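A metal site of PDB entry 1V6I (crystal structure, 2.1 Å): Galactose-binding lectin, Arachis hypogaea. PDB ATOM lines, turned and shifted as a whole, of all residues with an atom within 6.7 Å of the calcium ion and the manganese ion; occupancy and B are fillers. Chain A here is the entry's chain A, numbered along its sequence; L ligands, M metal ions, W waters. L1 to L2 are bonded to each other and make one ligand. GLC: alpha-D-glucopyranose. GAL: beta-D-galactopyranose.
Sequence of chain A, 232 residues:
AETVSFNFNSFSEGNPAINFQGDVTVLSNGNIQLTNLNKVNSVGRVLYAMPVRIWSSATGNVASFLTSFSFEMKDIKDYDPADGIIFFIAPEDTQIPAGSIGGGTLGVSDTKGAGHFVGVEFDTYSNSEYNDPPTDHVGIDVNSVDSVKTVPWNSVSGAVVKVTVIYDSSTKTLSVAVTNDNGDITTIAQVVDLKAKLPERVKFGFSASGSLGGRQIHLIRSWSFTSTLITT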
ATOM      1  N   ASP A  83     -17.396 -23.795 -11.113  1.00  0.00           N
ATOM      2  CA  ASP A  83     -18.128 -22.528 -11.260  1.00  0.00           C
ATOM      3  C   ASP A  83     -17.351 -21.334 -10.716  1.00  0.00           C
ATOM      4  O   ASP A  83     -17.578 -20.193 -11.128  1.00  0.00           O
ATOM      5  CB  ASP A  83     -19.475 -22.609 -10.550  1.00  0.00           C
ATOM      6  CG  ASP A  83     -20.593 -23.086 -11.459  1.00  0.00           C
ATOM      7  OD1 ASP A  83     -21.105 -22.275 -12.245  1.00  0.00           O
ATOM      8  OD2 ASP A  83     -20.954 -24.280 -11.379  1.00  0.00           O
ATOM      9  N   GLY A 103     -23.608 -24.875  -8.529  1.00  0.00           N
ATOM     10  CA  GLY A 103     -23.479 -24.138  -9.765  1.00  0.00           C
ATOM     11  C   GLY A 103     -23.202 -22.651  -9.616  1.00  0.00           C
ATOM     12  O   GLY A 103     -22.338 -22.248  -8.829  1.00  0.00           O
ATOM     13  N   GLY A 104     -23.955 -21.840 -10.357  1.00  0.00           N
ATOM     14  CA  GLY A 104     -23.790 -20.402 -10.318  1.00  0.00           C
ATOM     15  C   GLY A 104     -24.129 -19.688  -9.018  1.00  0.00           C
ATOM     16  O   GLY A 104     -23.849 -18.498  -8.883  1.00  0.00           O
ATOM     17  N   THR A 105     -24.733 -20.394  -8.070  1.00  0.00           N
ATOM     18  CA  THR A 105     -25.093 -19.775  -6.798  1.00  0.00           C
ATOM     19  C   THR A 105     -23.846 -19.651  -5.917  1.00  0.00           C
ATOM     20  O   THR A 105     -23.862 -18.994  -4.887  1.00  0.00           O
ATOM     21  CB  THR A 105     -26.152 -20.608  -6.022  1.00  0.00           C
ATOM     22  OG1 THR A 105     -25.553 -21.817  -5.549  1.00  0.00           O
ATOM     23  CG2 THR A 105     -27.317 -20.954  -6.939  1.00  0.00           C
ATOM     24  N   LEU A 106     -22.765 -20.304  -6.352  1.00  0.00           N
ATOM     25  CA  LEU A 106     -21.491 -20.304  -5.661  1.00  0.00           C
ATOM     26  C   LEU A 106     -21.551 -20.768  -4.208  1.00  0.00           C
ATOM     27  O   LEU A 106     -20.651 -20.478  -3.407  1.00  0.00           O
ATOM     28  CB  LEU A 106     -20.851 -18.897  -5.757  1.00  0.00           C
ATOM     29  CG  LEU A 106     -20.538 -18.476  -7.206  1.00  0.00           C
ATOM     30  CD1 LEU A 106     -19.942 -17.083  -7.244  1.00  0.00           C
ATOM     31  CD2 LEU A 106     -19.574 -19.464  -7.827  1.00  0.00           C
ATOM     32  N   GLU A 121     -16.307 -12.343  -5.703  1.00  0.00           N
ATOM     33  CA  GLU A 121     -16.319 -13.585  -6.467  1.00  0.00           C
ATOM     34  C   GLU A 121     -15.311 -13.647  -7.605  1.00  0.00           C
ATOM     35  O   GLU A 121     -14.959 -12.629  -8.226  1.00  0.00           O
ATOM     36  CB  GLU A 121     -17.725 -13.846  -7.020  1.00  0.00           C
ATOM     37  CG  GLU A 121     -18.241 -12.760  -7.935  1.00  0.00           C
ATOM     38  CD  GLU A 121     -19.463 -13.189  -8.724  1.00  0.00           C
ATOM     39  OE1 GLU A 121     -20.484 -13.541  -8.114  1.00  0.00           O
ATOM     40  OE2 GLU A 121     -19.384 -13.172  -9.965  1.00  0.00           O
ATOM     41  N   ASP A 123     -15.497 -15.647 -10.586  1.00  0.00           N
ATOM     42  CA  ASP A 123     -16.443 -16.391 -11.387  1.00  0.00           C
ATOM     43  C   ASP A 123     -15.932 -16.919 -12.730  1.00  0.00           C
ATOM     44  O   ASP A 123     -15.564 -16.130 -13.599  1.00  0.00           O
ATOM     45  CB  ASP A 123     -17.642 -15.477 -11.621  1.00  0.00           C
ATOM     46  CG  ASP A 123     -18.882 -16.242 -11.861  1.00  0.00           C
ATOM     47  OD1 ASP A 123     -18.784 -17.365 -12.394  1.00  0.00           O
ATOM     48  OD2 ASP A 123     -19.962 -15.713 -11.520  1.00  0.00           O
ATOM     49  N   THR A 124     -15.967 -18.237 -12.908  1.00  0.00           N
ATOM     50  CA  THR A 124     -15.463 -18.838 -14.145  1.00  0.00           C
ATOM     51  C   THR A 124     -16.500 -19.337 -15.151  1.00  0.00           C
ATOM     52  O   THR A 124     -16.146 -19.955 -16.140  1.00  0.00           O
ATOM     53  CB  THR A 124     -14.521 -20.018 -13.830  1.00  0.00           C
ATOM     54  OG1 THR A 124     -15.287 -21.096 -13.287  1.00  0.00           O
ATOM     55  CG2 THR A 124     -13.455 -19.594 -12.824  1.00  0.00           C
ATOM     56  N   TYR A 125     -17.773 -19.091 -14.898  1.00  0.00           N
ATOM     57  CA  TYR A 125     -18.809 -19.527 -15.850  1.00  0.00           C
ATOM     58  C   TYR A 125     -19.879 -18.454 -15.963  1.00  0.00           C
ATOM     59  O   TYR A 125     -20.277 -17.877 -14.962  1.00  0.00           O
ATOM     60  CB  TYR A 125     -19.440 -20.850 -15.416  1.00  0.00           C
ATOM     61  CG  TYR A 125     -20.550 -21.278 -16.345  1.00  0.00           C
ATOM     62  CD1 TYR A 125     -21.850 -20.791 -16.177  1.00  0.00           C
ATOM     63  CD2 TYR A 125     -20.294 -22.120 -17.434  1.00  0.00           C
ATOM     64  CE1 TYR A 125     -22.861 -21.120 -17.068  1.00  0.00           C
ATOM     65  CE2 TYR A 125     -21.303 -22.456 -18.332  1.00  0.00           C
ATOM     66  CZ  TYR A 125     -22.581 -21.951 -18.144  1.00  0.00           C
ATOM     67  OH  TYR A 125     -23.581 -22.272 -19.025  1.00  0.00           O
ATOM     68  N   SER A 126     -20.364 -18.193 -17.164  1.00  0.00           N
ATOM     69  CA  SER A 126     -21.359 -17.145 -17.328  1.00  0.00           C
ATOM     70  C   SER A 126     -22.810 -17.585 -17.210  1.00  0.00           C
ATOM     71  O   SER A 126     -23.382 -18.119 -18.155  1.00  0.00           O
ATOM     72  CB  SER A 126     -21.137 -16.455 -18.675  1.00  0.00           C
ATOM     73  OG  SER A 126     -22.101 -15.438 -18.884  1.00  0.00           O
ATOM     74  N   ASN A 127     -23.403 -17.357 -16.031  1.00  0.00           N
ATOM     75  CA  ASN A 127     -24.810 -17.711 -15.807  1.00  0.00           C
ATOM     76  C   ASN A 127     -25.653 -16.512 -16.195  1.00  0.00           C
ATOM     77  O   ASN A 127     -25.686 -15.506 -15.485  1.00  0.00           O
ATOM     78  CB  ASN A 127     -25.095 -18.032 -14.334  1.00  0.00           C
ATOM     79  CG  ASN A 127     -24.360 -19.256 -13.839  1.00  0.00           C
ATOM     80  OD1 ASN A 127     -23.179 -19.190 -13.524  1.00  0.00           O
ATOM     81  ND2 ASN A 127     -25.051 -20.384 -13.787  1.00  0.00           N
ATOM     82  N   TYR A 130     -28.195 -14.912 -13.818  1.00  0.00           N
ATOM     83  CA  TYR A 130     -27.728 -14.005 -12.752  1.00  0.00           C
ATOM     84  C   TYR A 130     -27.040 -12.793 -13.377  1.00  0.00           C
ATOM     85  O   TYR A 130     -26.251 -12.114 -12.732  1.00  0.00           O
ATOM     86  CB  TYR A 130     -26.758 -14.723 -11.817  1.00  0.00           C
ATOM     87  CG  TYR A 130     -27.329 -15.963 -11.177  1.00  0.00           C
ATOM     88  CD1 TYR A 130     -28.557 -15.940 -10.533  1.00  0.00           C
ATOM     89  CD2 TYR A 130     -26.651 -17.186 -11.248  1.00  0.00           C
ATOM     90  CE1 TYR A 130     -29.112 -17.091  -9.983  1.00  0.00           C
ATOM     91  CE2 TYR A 130     -27.194 -18.346 -10.684  1.00  0.00           C
ATOM     92  CZ  TYR A 130     -28.427 -18.292 -10.060  1.00  0.00           C
ATOM     93  OH  TYR A 130     -28.986 -19.429  -9.526  1.00  0.00           O
ATOM     94  N   ASN A 131     -27.358 -12.550 -14.647  1.00  0.00           N
ATOM     95  CA  ASN A 131     -26.811 -11.426 -15.398  1.00  0.00           C
ATOM     96  C   ASN A 131     -25.285 -11.332 -15.405  1.00  0.00           C
ATOM     97  O   ASN A 131     -24.719 -10.249 -15.335  1.00  0.00           O
ATOM     98  CB  ASN A 131     -27.402 -10.113 -14.877  1.00  0.00           C
ATOM     99  CG  ASN A 131     -28.919 -10.095 -14.939  1.00  0.00           C
ATOM    100  OD1 ASN A 131     -29.500 -10.445 -15.963  1.00  0.00           O
ATOM    101  ND2 ASN A 131     -29.560  -9.677 -13.860  1.00  0.00           N
ATOM    102  N   ASP A 132     -24.626 -12.491 -15.506  1.00  0.00           N
ATOM    103  CA  ASP A 132     -23.170 -12.528 -15.536  1.00  0.00           C
ATOM    104  C   ASP A 132     -22.590 -11.907 -16.795  1.00  0.00           C
ATOM    105  O   ASP A 132     -23.236 -11.892 -17.840  1.00  0.00           O
ATOM    106  CB  ASP A 132     -22.659 -13.969 -15.513  1.00  0.00           C
ATOM    107  CG  ASP A 132     -22.472 -14.507 -14.129  1.00  0.00           C
ATOM    108  OD1 ASP A 132     -22.174 -13.719 -13.212  1.00  0.00           O
ATOM    109  OD2 ASP A 132     -22.597 -15.727 -13.962  1.00  0.00           O
ATOM    110  N   PRO A 133     -21.359 -11.388 -16.703  1.00  0.00           N
ATOM    111  CA  PRO A 133     -20.755 -10.801 -17.902  1.00  0.00           C
ATOM    112  C   PRO A 133     -20.466 -12.017 -18.775  1.00  0.00           C
ATOM    113  O   PRO A 133     -20.557 -13.154 -18.307  1.00  0.00           O
ATOM    114  CB  PRO A 133     -19.476 -10.159 -17.364  1.00  0.00           C
ATOM    115  CG  PRO A 133     -19.819  -9.841 -15.946  1.00  0.00           C
ATOM    116  CD  PRO A 133     -20.565 -11.073 -15.502  1.00  0.00           C
ATOM    117  N   HIS A 137     -14.783 -13.400 -14.614  1.00  0.00           N
ATOM    118  CA  HIS A 137     -14.766 -12.087 -14.000  1.00  0.00           C
ATOM    119  C   HIS A 137     -14.658 -12.085 -12.483  1.00  0.00           C
ATOM    120  O   HIS A 137     -14.854 -13.093 -11.814  1.00  0.00           O
ATOM    121  CB  HIS A 137     -16.050 -11.344 -14.372  1.00  0.00           C
ATOM    122  CG  HIS A 137     -17.289 -12.115 -14.062  1.00  0.00           C
ATOM    123  ND1 HIS A 137     -17.706 -13.190 -14.824  1.00  0.00           N
ATOM    124  CD2 HIS A 137     -18.165 -12.011 -13.039  1.00  0.00           C
ATOM    125  CE1 HIS A 137     -18.793 -13.714 -14.268  1.00  0.00           C
ATOM    126  NE2 HIS A 137     -19.091 -13.017 -13.190  1.00  0.00           N
ATOM    127  N   VAL A 138     -14.331 -10.905 -11.956  1.00  0.00           N
ATOM    128  CA  VAL A 138     -14.250 -10.696 -10.519  1.00  0.00           C
ATOM    129  C   VAL A 138     -15.426  -9.756 -10.258  1.00  0.00           C
ATOM    130  O   VAL A 138     -15.671  -8.827 -11.039  1.00  0.00           O
ATOM    131  CB  VAL A 138     -12.937  -9.997 -10.120  1.00  0.00           C
ATOM    132  CG1 VAL A 138     -12.923  -9.747  -8.614  1.00  0.00           C
ATOM    133  CG2 VAL A 138     -11.744 -10.857 -10.519  1.00  0.00           C
ATOM    134  N   GLY A 139     -16.171  -9.993  -9.200  1.00  0.00           N
ATOM    135  CA  GLY A 139     -17.299  -9.131  -8.928  1.00  0.00           C
ATOM    136  C   GLY A 139     -17.523  -8.909  -7.454  1.00  0.00           C
ATOM    137  O   GLY A 139     -17.084  -9.702  -6.623  1.00  0.00           O
ATOM    138  N   ASP A 141     -20.266  -8.738  -4.699  1.00  0.00           N
ATOM    139  CA  ASP A 141     -21.627  -9.179  -4.455  1.00  0.00           C
ATOM    140  C   ASP A 141     -22.183  -8.686  -3.123  1.00  0.00           C
ATOM    141  O   ASP A 141     -21.519  -8.784  -2.088  1.00  0.00           O
ATOM    142  CB  ASP A 141     -21.706 -10.712  -4.481  1.00  0.00           C
ATOM    143  CG  ASP A 141     -21.300 -11.307  -5.822  1.00  0.00           C
ATOM    144  OD1 ASP A 141     -21.211 -10.586  -6.830  1.00  0.00           O
ATOM    145  OD2 ASP A 141     -21.070 -12.543  -5.867  1.00  0.00           O
ATOM    146  N   VAL A 145     -25.794 -12.945  -6.208  1.00  0.00           N
ATOM    147  CA  VAL A 145     -24.707 -13.322  -7.102  1.00  0.00           C
ATOM    148  C   VAL A 145     -24.838 -12.504  -8.386  1.00  0.00           C
ATOM    149  O   VAL A 145     -24.066 -12.657  -9.336  1.00  0.00           O
ATOM    150  CB  VAL A 145     -24.718 -14.828  -7.433  1.00  0.00           C
ATOM    151  CG1 VAL A 145     -24.270 -15.634  -6.208  1.00  0.00           C
ATOM    152  CG2 VAL A 145     -26.093 -15.257  -7.886  1.00  0.00           C
ATOM    153  N   ASP A 146     -25.854 -11.654  -8.408  1.00  0.00           N
ATOM    154  CA  ASP A 146     -26.053 -10.742  -9.530  1.00  0.00           C
ATOM    155  C   ASP A 146     -25.219  -9.576  -9.024  1.00  0.00           C
ATOM    156  O   ASP A 146     -25.709  -8.695  -8.322  1.00  0.00           O
ATOM    157  CB  ASP A 146     -27.520 -10.321  -9.642  1.00  0.00           C
ATOM    158  CG  ASP A 146     -27.780  -9.473 -10.870  1.00  0.00           C
ATOM    159  OD1 ASP A 146     -26.875  -8.721 -11.301  1.00  0.00           O
ATOM    160  OD2 ASP A 146     -28.897  -9.539 -11.417  1.00  0.00           O
ATOM    161  N   SER A 147     -23.933  -9.605  -9.370  1.00  0.00           N
ATOM    162  CA  SER A 147     -22.972  -8.593  -8.924  1.00  0.00           C
ATOM    163  C   SER A 147     -23.366  -7.131  -9.107  1.00  0.00           C
ATOM    164  O   SER A 147     -23.941  -6.730 -10.114  1.00  0.00           O
ATOM    165  CB  SER A 147     -21.623  -8.826  -9.616  1.00  0.00           C
ATOM    166  OG  SER A 147     -21.113 -10.121  -9.325  1.00  0.00           O
ATOM    167  N   THR A 150     -18.684  -5.692 -11.714  1.00  0.00           N
ATOM    168  CA  THR A 150     -17.749  -6.724 -12.163  1.00  0.00           C
ATOM    169  C   THR A 150     -16.661  -6.117 -13.019  1.00  0.00           C
ATOM    170  O   THR A 150     -16.800  -4.992 -13.501  1.00  0.00           O
ATOM    171  CB  THR A 150     -18.428  -7.826 -13.010  1.00  0.00           C
ATOM    172  OG1 THR A 150     -18.845  -7.261 -14.268  1.00  0.00           O
ATOM    173  CG2 THR A 150     -19.637  -8.410 -12.285  1.00  0.00           C
HETATM  174  C1  GLC L   1     -27.607 -29.358 -17.637  1.00  0.00           C
HETATM  175  C2  GLC L   1     -26.135 -29.587 -17.261  1.00  0.00           C
HETATM  176  C3  GLC L   1     -25.725 -28.676 -16.099  1.00  0.00           C
HETATM  177  C4  GLC L   1     -26.063 -27.229 -16.427  1.00  0.00           C
HETATM  178  C5  GLC L   1     -27.555 -27.128 -16.764  1.00  0.00           C
HETATM  179  C6  GLC L   1     -28.010 -25.723 -17.106  1.00  0.00           C
HETATM  180  O1  GLC L   1     -28.422 -29.752 -16.588  1.00  0.00           O
HETATM  181  O2  GLC L   1     -25.961 -30.943 -16.881  1.00  0.00           O
HETATM  182  O3  GLC L   1     -24.327 -28.795 -15.868  1.00  0.00           O
HETATM  183  O4  GLC L   1     -25.754 -26.393 -15.299  1.00  0.00           O
HETATM  184  O5  GLC L   1     -27.864 -27.964 -17.892  1.00  0.00           O
HETATM  185  O6  GLC L   1     -27.183 -25.152 -18.097  1.00  0.00           O
HETATM  186  C1  GAL L   2     -24.869 -25.353 -15.516  1.00  0.00           C
HETATM  187  C2  GAL L   2     -24.763 -24.515 -14.241  1.00  0.00           C
HETATM  188  C3  GAL L   2     -23.654 -23.466 -14.367  1.00  0.00           C
HETATM  189  C4  GAL L   2     -22.335 -24.146 -14.775  1.00  0.00           C
HETATM  190  C5  GAL L   2     -22.581 -24.912 -16.074  1.00  0.00           C
HETATM  191  C6  GAL L   2     -21.340 -25.617 -16.591  1.00  0.00           C
HETATM  192  O2  GAL L   2     -25.997 -23.863 -13.997  1.00  0.00           O
HETATM  193  O3  GAL L   2     -23.492 -22.798 -13.131  1.00  0.00           O
HETATM  194  O4  GAL L   2     -21.922 -25.053 -13.759  1.00  0.00           O
HETATM  195  O5  GAL L   2     -23.587 -25.910 -15.857  1.00  0.00           O
HETATM  196  O6  GAL L   2     -21.459 -25.905 -17.973  1.00  0.00           O
HETATM  197 CA    CA M   1     -21.354 -17.565 -12.757  1.00  0.00          CA
HETATM  198 MN    MN M   2     -20.681 -13.629 -11.643  1.00  0.00          MN
HETATM  199  O   HOH W   1     -21.380 -11.404 -11.591  1.00  0.00           O
HETATM  200  O   HOH W   2     -22.157 -14.356  -9.990  1.00  0.00           O
HETATM  201  O   HOH W   3     -22.751 -16.902 -10.715  1.00  0.00           O
HETATM  202  O   HOH W   4     -20.417 -19.771 -11.817  1.00  0.00           O
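An oxygen (O3) of GAL L2 is in hydrogen-bond range of the side-chain amide nitrogen (ND2) of Asn 127 (2.9 Å). The backbone NH (N) of Gly 104 sits at hydrogen-bond distance from an oxygen (O3) of GAL L2 (3.0 Å). OD1 of Asp 83 is in hydrogen-bond range of O3 of GAL L2, at 2.6 Å.
OE1 of Glu 121 lies close to OD2 of Asp 141 (2.5 Å). N of Glu 121 lies within hydrogen-bond range of O of Gly 139, 2.9 Å away.
Within 4 Å of the calcium ion: Asp 123, Tyr 125, Asn 127 and Asp 132. The nearest printed residue that does not touch the calcium ion is Gly 104 (4.5 Å).
Four residues have an atom within 4 Å of the manganese ion: Glu 121, Asp 123, Asp 132 and His 137. The nearest printed residue that does not touch the manganese ion is Val 145 (4.2 Å).
The calcium ion is bound by O of Tyr 125 (2.5 Å), OD2 of Asp 132 (2.5 Å), OD1 of Asn 127 (2.6 Å), water W3 (2.6 Å), water W4 (2.6 Å), OD1 of Asp 123 (2.6 Å) and OD2 of Asp 123 (2.6 Å).
The manganese ion is bound by the side-chain carboxylate (OD1) of Asp 132 (2.2 Å). OE2 of Glu 121 is bound to the manganese ion, at 2.2 Å. OD2 of Asp 123 binds the manganese ion (2.2 Å). A ring nitrogen (NE2) of His 137 binds the manganese ion, at 2.3 Å. Water W1 binds the manganese ion, at 2.3 Å. The manganese ion is bound by water W2, at 2.3 Å. The manganese ion has six donor atoms within binding distance.
Water W2 lies within hydrogen-bond range of O of Val 145 (2.6 Å) and OE1 of Glu 121 (2.6 Å).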
